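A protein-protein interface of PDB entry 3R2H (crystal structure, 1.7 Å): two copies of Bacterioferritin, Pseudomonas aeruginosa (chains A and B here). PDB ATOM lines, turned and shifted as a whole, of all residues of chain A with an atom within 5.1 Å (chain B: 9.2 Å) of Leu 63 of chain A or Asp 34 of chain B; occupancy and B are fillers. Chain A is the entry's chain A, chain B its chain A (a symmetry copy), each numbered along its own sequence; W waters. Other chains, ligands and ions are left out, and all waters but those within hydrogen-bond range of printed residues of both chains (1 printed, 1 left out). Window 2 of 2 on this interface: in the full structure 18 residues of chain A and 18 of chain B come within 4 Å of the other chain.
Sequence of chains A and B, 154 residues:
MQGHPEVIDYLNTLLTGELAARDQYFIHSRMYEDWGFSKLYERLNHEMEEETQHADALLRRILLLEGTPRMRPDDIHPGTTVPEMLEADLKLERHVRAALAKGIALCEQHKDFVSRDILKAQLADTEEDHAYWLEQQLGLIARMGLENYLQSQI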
ATOM      1  N   LEU A  58       8.950   0.962  17.838  1.00  0.00           N
ATOM      2  CA  LEU A  58       8.398  -0.242  17.182  1.00  0.00           C
ATOM      3  C   LEU A  58       6.974  -0.027  16.673  1.00  0.00           C
ATOM      4  O   LEU A  58       6.636  -0.380  15.528  1.00  0.00           O
ATOM      5  CB  LEU A  58       8.368  -1.426  18.171  1.00  0.00           C
ATOM      6  CG  LEU A  58       9.763  -1.879  18.607  1.00  0.00           C
ATOM      7  CD1 LEU A  58       9.692  -2.877  19.792  1.00  0.00           C
ATOM      8  CD2 LEU A  58      10.560  -2.544  17.483  1.00  0.00           C
ATOM      9  N   LEU A  59       6.137   0.568  17.518  1.00  0.00           N
ATOM     10  CA  LEU A  59       4.769   0.870  17.129  1.00  0.00           C
ATOM     11  C   LEU A  59       4.740   1.720  15.856  1.00  0.00           C
ATOM     12  O   LEU A  59       4.017   1.409  14.907  1.00  0.00           O
ATOM     13  CB  LEU A  59       4.094   1.591  18.305  1.00  0.00           C
ATOM     14  CG  LEU A  59       2.576   1.796  18.290  1.00  0.00           C
ATOM     15  CD1 LEU A  59       2.167   2.303  19.648  1.00  0.00           C
ATOM     16  CD2 LEU A  59       2.188   2.779  17.259  1.00  0.00           C
ATOM     17  N   ARG A  60       5.544   2.779  15.811  1.00  0.00           N
ATOM     18  CA  ARG A  60       5.521   3.644  14.644  1.00  0.00           C
ATOM     19  C   ARG A  60       6.006   2.927  13.402  1.00  0.00           C
ATOM     20  O   ARG A  60       5.491   3.163  12.316  1.00  0.00           O
ATOM     21  CB  ARG A  60       6.386   4.867  14.874  1.00  0.00           C
ATOM     22  CG  ARG A  60       5.720   5.876  15.833  1.00  0.00           C
ATOM     23  CD  ARG A  60       6.690   6.989  16.086  1.00  0.00           C
ATOM     24  NE  ARG A  60       6.284   7.863  17.173  1.00  0.00           N
ATOM     25  CZ  ARG A  60       5.858   9.097  17.009  1.00  0.00           C
ATOM     26  NH1 ARG A  60       5.759   9.598  15.799  1.00  0.00           N
ATOM     27  NH2 ARG A  60       5.547   9.833  18.060  1.00  0.00           N
ATOM     28  N   ARG A  61       6.994   2.053  13.550  1.00  0.00           N
ATOM     29  CA  ARG A  61       7.525   1.307  12.405  1.00  0.00           C
ATOM     30  C   ARG A  61       6.462   0.338  11.869  1.00  0.00           C
ATOM     31  O   ARG A  61       6.309   0.164  10.652  1.00  0.00           O
ATOM     32  CB  ARG A  61       8.792   0.542  12.830  1.00  0.00           C
ATOM     33  CG  ARG A  61       9.416  -0.301  11.699  1.00  0.00           C
ATOM     34  CD  ARG A  61       9.950   0.623  10.570  1.00  0.00           C
ATOM     35  NE  ARG A  61      10.604  -0.171   9.530  1.00  0.00           N
ATOM     36  CZ  ARG A  61      10.922   0.306   8.331  1.00  0.00           C
ATOM     37  NH1 ARG A  61      10.714   1.600   8.035  1.00  0.00           N
ATOM     38  NH2 ARG A  61      11.464  -0.511   7.431  1.00  0.00           N
ATOM     39  N   ILE A  62       5.741  -0.309  12.774  1.00  0.00           N
ATOM     40  CA  ILE A  62       4.688  -1.254  12.367  1.00  0.00           C
ATOM     41  C   ILE A  62       3.607  -0.519  11.583  1.00  0.00           C
ATOM     42  O   ILE A  62       3.175  -1.007  10.532  1.00  0.00           O
ATOM     43  CB  ILE A  62       4.100  -1.946  13.611  1.00  0.00           C
ATOM     44  CG1 ILE A  62       5.152  -2.884  14.222  1.00  0.00           C
ATOM     45  CG2 ILE A  62       2.825  -2.702  13.267  1.00  0.00           C
ATOM     46  CD1 ILE A  62       4.854  -3.220  15.702  1.00  0.00           C
ATOM     47  N   LEU A  63       3.189   0.660  12.060  1.00  0.00           N
ATOM     48  CA  LEU A  63       2.193   1.459  11.318  1.00  0.00           C
ATOM     49  C   LEU A  63       2.745   1.894   9.949  1.00  0.00           C
ATOM     50  O   LEU A  63       2.038   1.850   8.925  1.00  0.00           O
ATOM     51  CB  LEU A  63       1.791   2.710  12.136  1.00  0.00           C
ATOM     52  CG  LEU A  63       0.933   2.399  13.370  1.00  0.00           C
ATOM     53  CD1 LEU A  63       0.713   3.692  14.200  1.00  0.00           C
ATOM     54  CD2 LEU A  63      -0.447   1.803  12.956  1.00  0.00           C
ATOM     55  N   LEU A  64       4.014   2.301   9.915  1.00  0.00           N
ATOM     56  CA  LEU A  64       4.594   2.767   8.670  1.00  0.00           C
ATOM     57  C   LEU A  64       4.540   1.627   7.648  1.00  0.00           C
ATOM     58  O   LEU A  64       4.253   1.858   6.473  1.00  0.00           O
ATOM     59  CB  LEU A  64       6.035   3.236   8.909  1.00  0.00           C
ATOM     60  CG  LEU A  64       6.826   3.768   7.695  1.00  0.00           C
ATOM     61  CD1 LEU A  64       7.927   4.705   8.174  1.00  0.00           C
ATOM     62  CD2 LEU A  64       7.415   2.585   6.902  1.00  0.00           C
ATOM     63  N   LEU A  65       4.784   0.402   8.115  1.00  0.00           N
ATOM     64  CA  LEU A  65       4.791  -0.804   7.271  1.00  0.00           C
ATOM     65  C   LEU A  65       3.378  -1.320   7.021  1.00  0.00           C
ATOM     66  O   LEU A  65       3.214  -2.430   6.489  1.00  0.00           O
ATOM     67  CB  LEU A  65       5.619  -1.901   7.949  1.00  0.00           C
ATOM     68  CG  LEU A  65       7.113  -1.554   8.084  1.00  0.00           C
ATOM     69  CD1 LEU A  65       7.819  -2.702   8.793  1.00  0.00           C
ATOM     70  CD2 LEU A  65       7.741  -1.268   6.719  1.00  0.00           C
ATOM     71  N   GLU A  66       2.376  -0.518   7.409  1.00  0.00           N
ATOM     72  CA  GLU A  66       0.946  -0.835   7.200  1.00  0.00           C
ATOM     73  C   GLU A  66       0.429  -2.039   8.000  1.00  0.00           C
ATOM     74  O   GLU A  66      -0.578  -2.679   7.640  1.00  0.00           O
ATOM     75  CB  GLU A  66       0.633  -0.974   5.697  1.00  0.00           C
ATOM     76  CG  GLU A  66       1.067   0.262   4.904  1.00  0.00           C
ATOM     77  CD  GLU A  66       0.683   0.219   3.445  1.00  0.00           C
ATOM     78  OE1 GLU A  66      -0.269  -0.519   3.107  1.00  0.00           O
ATOM     79  OE2 GLU A  66       1.329   0.940   2.637  1.00  0.00           O
ATOM     80  N   GLY A  67       1.117  -2.338   9.092  1.00  0.00           N
ATOM     81  CA  GLY A  67       0.699  -3.379   9.994  1.00  0.00           C
ATOM     82  C   GLY A  67      -0.184  -2.806  11.077  1.00  0.00           C
ATOM     83  O   GLY A  67      -0.354  -1.592  11.183  1.00  0.00           O
ATOM     84  N   PRO A  69      -0.596  -2.607  15.152  1.00  0.00           N
ATOM     85  CA  PRO A  69       0.172  -2.943  16.353  1.00  0.00           C
ATOM     86  C   PRO A  69      -0.627  -3.738  17.349  1.00  0.00           C
ATOM     87  O   PRO A  69      -1.818  -3.504  17.503  1.00  0.00           O
ATOM     88  CB  PRO A  69       0.541  -1.572  16.949  1.00  0.00           C
ATOM     89  CG  PRO A  69       0.611  -0.668  15.714  1.00  0.00           C
ATOM     90  CD  PRO A  69      -0.518  -1.155  14.853  1.00  0.00           C
ATOM     91  N   PHE B  26      -2.072   5.862  23.343  1.00  0.00           N
ATOM     92  CA  PHE B  26      -0.775   5.588  22.692  1.00  0.00           C
ATOM     93  C   PHE B  26      -1.036   5.144  21.251  1.00  0.00           C
ATOM     94  O   PHE B  26      -0.529   5.740  20.305  1.00  0.00           O
ATOM     95  CB  PHE B  26      -0.076   4.477  23.509  1.00  0.00           C
ATOM     96  CG  PHE B  26       1.428   4.298  23.272  1.00  0.00           C
ATOM     97  CD1 PHE B  26       2.102   3.336  24.012  1.00  0.00           C
ATOM     98  CD2 PHE B  26       2.149   5.042  22.343  1.00  0.00           C
ATOM     99  CE1 PHE B  26       3.474   3.140  23.868  1.00  0.00           C
ATOM    100  CE2 PHE B  26       3.527   4.848  22.192  1.00  0.00           C
ATOM    101  CZ  PHE B  26       4.188   3.918  22.940  1.00  0.00           C
ATOM    102  N   ILE B  27      -1.846   4.106  21.054  1.00  0.00           N
ATOM    103  CA  ILE B  27      -2.054   3.632  19.691  1.00  0.00           C
ATOM    104  C   ILE B  27      -2.841   4.643  18.865  1.00  0.00           C
ATOM    105  O   ILE B  27      -2.467   4.926  17.732  1.00  0.00           O
ATOM    106  CB  ILE B  27      -2.683   2.194  19.618  1.00  0.00           C
ATOM    107  CG1 ILE B  27      -2.850   1.749  18.171  1.00  0.00           C
ATOM    108  CG2 ILE B  27      -4.039   2.091  20.328  1.00  0.00           C
ATOM    109  CD1 ILE B  27      -1.587   1.740  17.398  1.00  0.00           C
ATOM    110  N   HIS B  28      -3.906   5.229  19.408  1.00  0.00           N
ATOM    111  CA  HIS B  28      -4.656   6.233  18.605  1.00  0.00           C
ATOM    112  C   HIS B  28      -3.796   7.446  18.211  1.00  0.00           C
ATOM    113  O   HIS B  28      -3.844   7.874  17.071  1.00  0.00           O
ATOM    114  CB  HIS B  28      -5.899   6.737  19.346  1.00  0.00           C
ATOM    115  CG  HIS B  28      -7.058   5.776  19.317  1.00  0.00           C
ATOM    116  ND1 HIS B  28      -8.181   5.952  20.100  1.00  0.00           N
ATOM    117  CD2 HIS B  28      -7.267   4.647  18.598  1.00  0.00           C
ATOM    118  CE1 HIS B  28      -9.041   4.974  19.853  1.00  0.00           C
ATOM    119  NE2 HIS B  28      -8.509   4.169  18.952  1.00  0.00           N
ATOM    120  N   SER B  29      -3.004   7.994  19.131  1.00  0.00           N
ATOM    121  CA  SER B  29      -2.198   9.159  18.768  1.00  0.00           C
ATOM    122  C   SER B  29      -1.276   8.812  17.599  1.00  0.00           C
ATOM    123  O   SER B  29      -1.142   9.589  16.643  1.00  0.00           O
ATOM    124  CB  SER B  29      -1.406   9.668  19.981  1.00  0.00           C
ATOM    125  OG  SER B  29      -0.522   8.690  20.465  1.00  0.00           O
ATOM    126  N   ARG B  30      -0.645   7.638  17.639  1.00  0.00           N
ATOM    127  CA  ARG B  30       0.290   7.282  16.572  1.00  0.00           C
ATOM    128  C   ARG B  30      -0.432   6.951  15.263  1.00  0.00           C
ATOM    129  O   ARG B  30       0.113   7.207  14.189  1.00  0.00           O
ATOM    130  CB  ARG B  30       1.201   6.153  17.005  1.00  0.00           C
ATOM    131  CG  ARG B  30       2.453   6.660  17.758  1.00  0.00           C
ATOM    132  CD  ARG B  30       2.126   7.355  19.067  1.00  0.00           C
ATOM    133  NE  ARG B  30       3.360   7.703  19.787  1.00  0.00           N
ATOM    134  CZ  ARG B  30       3.385   8.536  20.819  1.00  0.00           C
ATOM    135  NH1 ARG B  30       2.257   9.114  21.241  1.00  0.00           N
ATOM    136  NH2 ARG B  30       4.528   8.793  21.440  1.00  0.00           N
ATOM    137  N   MET B  31      -1.645   6.411  15.351  1.00  0.00           N
ATOM    138  CA  MET B  31      -2.462   6.200  14.155  1.00  0.00           C
ATOM    139  C   MET B  31      -2.789   7.544  13.516  1.00  0.00           C
ATOM    140  O   MET B  31      -2.713   7.696  12.308  1.00  0.00           O
ATOM    141  CB  MET B  31      -3.762   5.476  14.494  1.00  0.00           C
ATOM    142  CG  MET B  31      -3.532   3.968  14.753  1.00  0.00           C
ATOM    143  SD  MET B  31      -5.005   3.167  15.404  1.00  0.00           S
ATOM    144  CE  MET B  31      -6.093   3.308  13.971  1.00  0.00           C
ATOM    145  N   TYR B  32      -3.164   8.526  14.330  1.00  0.00           N
ATOM    146  CA  TYR B  32      -3.475   9.854  13.816  1.00  0.00           C
ATOM    147  C   TYR B  32      -2.268  10.439  13.104  1.00  0.00           C
ATOM    148  O   TYR B  32      -2.409  11.064  12.052  1.00  0.00           O
ATOM    149  CB  TYR B  32      -3.893  10.784  14.974  1.00  0.00           C
ATOM    150  CG  TYR B  32      -5.282  10.533  15.537  1.00  0.00           C
ATOM    151  CD1 TYR B  32      -6.382  10.340  14.685  1.00  0.00           C
ATOM    152  CD2 TYR B  32      -5.518  10.585  16.901  1.00  0.00           C
ATOM    153  CE1 TYR B  32      -7.675  10.159  15.199  1.00  0.00           C
ATOM    154  CE2 TYR B  32      -6.814  10.407  17.430  1.00  0.00           C
ATOM    155  CZ  TYR B  32      -7.879  10.181  16.570  1.00  0.00           C
ATOM    156  OH  TYR B  32      -9.148  10.026  17.098  1.00  0.00           O
ATOM    157  N   GLU B  33      -1.084  10.253  13.676  1.00  0.00           N
ATOM    158  CA  GLU B  33       0.158  10.724  13.073  1.00  0.00           C
ATOM    159  C   GLU B  33       0.447  10.002  11.758  1.00  0.00           C
ATOM    160  O   GLU B  33       0.923  10.602  10.792  1.00  0.00           O
ATOM    161  CB  GLU B  33       1.317  10.476  14.037  1.00  0.00           C
ATOM    162  CG  GLU B  33       2.611  11.029  13.535  1.00  0.00           C
ATOM    163  CD  GLU B  33       2.768  12.493  13.899  1.00  0.00           C
ATOM    164  OE1 GLU B  33       3.801  12.826  14.520  1.00  0.00           O
ATOM    165  OE2 GLU B  33       1.859  13.303  13.590  1.00  0.00           O
ATOM    166  N   ASP B  34       0.174   8.698  11.741  1.00  0.00           N
ATOM    167  CA  ASP B  34       0.392   7.852  10.550  1.00  0.00           C
ATOM    168  C   ASP B  34      -0.421   8.393   9.361  1.00  0.00           C
ATOM    169  O   ASP B  34       0.015   8.309   8.213  1.00  0.00           O
ATOM    170  CB  ASP B  34      -0.001   6.412  10.889  1.00  0.00           C
ATOM    171  CG  ASP B  34       0.005   5.463   9.678  1.00  0.00           C
ATOM    172  OD1 ASP B  34       1.066   5.296   9.054  1.00  0.00           O
ATOM    173  OD2 ASP B  34      -1.044   4.815   9.423  1.00  0.00           O
ATOM    174  N   TRP B  35      -1.587   8.966   9.651  1.00  0.00           N
ATOM    175  CA  TRP B  35      -2.457   9.517   8.593  1.00  0.00           C
ATOM    176  C   TRP B  35      -2.192  10.992   8.296  1.00  0.00           C
ATOM    177  O   TRP B  35      -2.801  11.556   7.395  1.00  0.00           O
ATOM    178  CB  TRP B  35      -3.925   9.356   8.983  1.00  0.00           C
ATOM    179  CG  TRP B  35      -4.376   7.922   9.050  1.00  0.00           C
ATOM    180  CD1 TRP B  35      -3.907   6.865   8.312  1.00  0.00           C
ATOM    181  CD2 TRP B  35      -5.406   7.398   9.896  1.00  0.00           C
ATOM    182  NE1 TRP B  35      -4.582   5.707   8.663  1.00  0.00           N
ATOM    183  CE2 TRP B  35      -5.515   6.016   9.623  1.00  0.00           C
ATOM    184  CE3 TRP B  35      -6.259   7.973  10.855  1.00  0.00           C
ATOM    185  CZ2 TRP B  35      -6.420   5.183  10.300  1.00  0.00           C
ATOM    186  CZ3 TRP B  35      -7.159   7.147  11.517  1.00  0.00           C
ATOM    187  CH2 TRP B  35      -7.228   5.767  11.239  1.00  0.00           C
ATOM    188  N   GLY B  36      -1.340  11.635   9.082  1.00  0.00           N
ATOM    189  CA  GLY B  36      -0.999  13.032   8.829  1.00  0.00           C
ATOM    190  C   GLY B  36      -1.868  14.038   9.578  1.00  0.00           C
ATOM    191  O   GLY B  36      -1.880  15.210   9.215  1.00  0.00           O
ATOM    192  N   PHE B  37      -2.587  13.597  10.617  1.00  0.00           N
ATOM    193  CA  PHE B  37      -3.407  14.523  11.423  1.00  0.00           C
ATOM    194  C   PHE B  37      -2.637  14.933  12.676  1.00  0.00           C
ATOM    195  O   PHE B  37      -2.857  14.386  13.761  1.00  0.00           O
ATOM    196  CB  PHE B  37      -4.763  13.874  11.792  1.00  0.00           C
ATOM    197  CG  PHE B  37      -5.599  13.531  10.578  1.00  0.00           C
ATOM    198  CD1 PHE B  37      -5.998  14.534   9.704  1.00  0.00           C
ATOM    199  CD2 PHE B  37      -5.948  12.225  10.297  1.00  0.00           C
ATOM    200  CE1 PHE B  37      -6.730  14.225   8.556  1.00  0.00           C
ATOM    201  CE2 PHE B  37      -6.694  11.914   9.163  1.00  0.00           C
ATOM    202  CZ  PHE B  37      -7.071  12.926   8.292  1.00  0.00           C
ATOM    203  N   SER B  38      -1.724  15.887  12.521  1.00  0.00           N
ATOM    204  CA  SER B  38      -0.778  16.274  13.569  1.00  0.00           C
ATOM    205  C   SER B  38      -1.476  16.805  14.817  1.00  0.00           C
ATOM    206  O   SER B  38      -1.026  16.587  15.939  1.00  0.00           O
ATOM    207  CB  SER B  38       0.210  17.342  13.036  1.00  0.00           C
ATOM    208  OG  SER B  38      -0.368  18.638  13.013  1.00  0.00           O
ATOM    209  N   LEU B  40      -4.394  15.961  15.989  1.00  0.00           N
ATOM    210  CA  LEU B  40      -5.025  14.843  16.727  1.00  0.00           C
ATOM    211  C   LEU B  40      -3.949  14.011  17.413  1.00  0.00           C
ATOM    212  O   LEU B  40      -4.121  13.554  18.550  1.00  0.00           O
ATOM    213  CB  LEU B  40      -5.901  13.989  15.796  1.00  0.00           C
ATOM    214  CG  LEU B  40      -7.229  14.639  15.358  1.00  0.00           C
ATOM    215  CD1 LEU B  40      -7.902  13.794  14.296  1.00  0.00           C
ATOM    216  CD2 LEU B  40      -8.193  14.827  16.539  1.00  0.00           C
ATOM    217  N   TYR B  41      -2.809  13.838  16.750  1.00  0.00           N
ATOM    218  CA  TYR B  41      -1.661  13.183  17.396  1.00  0.00           C
ATOM    219  C   TYR B  41      -1.264  13.961  18.640  1.00  0.00           C
ATOM    220  O   TYR B  41      -1.064  13.383  19.712  1.00  0.00           O
ATOM    221  CB  TYR B  41      -0.454  13.142  16.452  1.00  0.00           C
ATOM    222  CG  TYR B  41       0.825  12.927  17.216  1.00  0.00           C
ATOM    223  CD1 TYR B  41       1.669  13.996  17.525  1.00  0.00           C
ATOM    224  CD2 TYR B  41       1.186  11.675  17.634  1.00  0.00           C
ATOM    225  CE1 TYR B  41       2.839  13.794  18.260  1.00  0.00           C
ATOM    226  CE2 TYR B  41       2.362  11.464  18.366  1.00  0.00           C
ATOM    227  CZ  TYR B  41       3.174  12.527  18.662  1.00  0.00           C
ATOM    228  OH  TYR B  41       4.320  12.302  19.386  1.00  0.00           O
ATOM    229  N   GLY B  79     -10.285   2.177  17.474  1.00  0.00           N
ATOM    230  CA  GLY B  79     -11.130   2.316  16.288  1.00  0.00           C
ATOM    231  C   GLY B  79     -10.298   2.185  15.034  1.00  0.00           C
ATOM    232  O   GLY B  79      -9.084   2.000  15.113  1.00  0.00           O
ATOM    233  N   THR B  80     -10.929   2.307  13.869  1.00  0.00           N
ATOM    234  CA  THR B  80     -10.207   2.121  12.606  1.00  0.00           C
ATOM    235  C   THR B  80     -10.302   3.325  11.685  1.00  0.00           C
ATOM    236  O   THR B  80      -9.657   3.343  10.625  1.00  0.00           O
ATOM    237  CB  THR B  80     -10.716   0.863  11.794  1.00  0.00           C
ATOM    238  OG1 THR B  80     -12.009   1.116  11.227  1.00  0.00           O
ATOM    239  CG2 THR B  80     -10.752  -0.371  12.676  1.00  0.00           C
ATOM    240  N   MET B  85     -12.471   6.273  16.283  1.00  0.00           N
ATOM    241  CA  MET B  85     -11.472   6.445  17.331  1.00  0.00           C
ATOM    242  C   MET B  85     -11.958   7.462  18.365  1.00  0.00           C
ATOM    243  O   MET B  85     -11.805   7.255  19.562  1.00  0.00           O
ATOM    244  CB  MET B  85     -10.115   6.866  16.731  1.00  0.00           C
ATOM    245  CG  MET B  85      -9.514   5.757  15.848  1.00  0.00           C
ATOM    246  SD  MET B  85      -8.400   6.431  14.593  1.00  0.00           S
ATOM    247  CE  MET B  85      -6.958   6.772  15.605  1.00  0.00           C
HETATM  248  O   HOH W   1      -0.698   2.059   8.804  1.00  0.00           O
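The side-chain hydroxyl (OG) of Ser 29 of chain B is in hydrogen-bond range of the backbone carbonyl oxygen (O) of Phe 26 of chain B, 3.0 Å away.
The side-chain hydroxyl of Ser 29 of chain B is in hydrogen-bond range of the guanidinium group of Arg 30 of chain B (2.9 Å).
Of the 18 printed residues of chain B, 7 touch a printed residue of chain A.
Hydrophobic or aromatic side chains of chain B that line the printed part of chain A: Phe 26, Ile 27 and Tyr 41.
Of the 11 printed residues of chain A, 4 touch a printed residue of chain B.
Hydrophobic or aromatic side chains of chain A that line the printed part of chain B: Leu 59, Leu 63 and Pro 69.
Among the printed residues, 10 pairs touch across the chains.
Among the printed residues, Asp or Glu carboxylates within 4 Å of a Lys or Arg side-chain nitrogen of the other chain: Arg 60 of chain A with Glu 33 of chain B (3.99 Å).
No position is printed for both chains.
Of the 10 pairs that touch across the chains among the printed residues, none has its exchanged pair printed and touching as well.
Water W1 lies within hydrogen-bond range of O of Leu 63 of chain A (2.7 Å) and OD2 of Asp 34 of chain B (2.8 Å).
Leu 59 of chain A touches Phe 26 of chain B (CD1 to CD2, 3.8 Å).
CD2 of Leu 59 of chain A touches CD1 of Ile 27 of chain B, at 3.9 Å.
Leu 59 of chain A touches Arg 30 of chain B.
Arg 60 of chain A touches Arg 30 of chain B (NH2 to NE, 3.5 Å).
O of Arg 30 of chain B touches CD1 of Leu 63 of chain A (3.6 Å).
Met 31 of chain B touches Leu 63 of chain A (N to CD1, 3.8 Å).
Leu 63 of chain A touches Asp 34 of chain B.
CG of Pro 69 of chain A touches CD1 of Ile 27 of chain B (3.7 Å).
The side-chain carboxylate (OE1) of Glu 33 of chain B lies within salt-bridge range of the guanidinium group (NH1) of Arg 60 of chain A, 3.99 Å away.
The guanidinium group of Arg 60 of chain A sits at hydrogen-bond distance from the side-chain hydroxyl of Tyr 41 of chain B, 3.1 Å away.
Leu 63 of chain A touches just these residues of chain B: Arg 30 (3.6 Å), Met 31 (3.8 Å) and Asp 34 (3.6 Å).
Of chain A, only Leu 63 (3.6 Å) comes within 4 Å of Asp 34 of chain B.
Printed residues of chain B within 4 Å of Leu 59 of chain A: Phe 26 (3.8 Å), Ile 27 (3.9 Å) and Arg 30 (3.5 Å).
Of the printed residues of chain B, Pro 69 of chain A touches Ile 27.
Printed residues of chain A within 4 Å of Met 31 of chain B: Leu 63.
Printed residues of chain A within 4 Å of Tyr 41 of chain B: Arg 60 (3.1 Å).
Of the printed residues of chain B, Arg 60 of chain A touches Arg 30, Glu 33 and Tyr 41.
The nearest residue of chain A that does not touch Asp 34 of chain B is Leu 64 of chain A (4.3 Å).
The nearest printed residue of chain A that does not touch Phe 26 of chain B is Arg 60 of chain A (6.5 Å).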
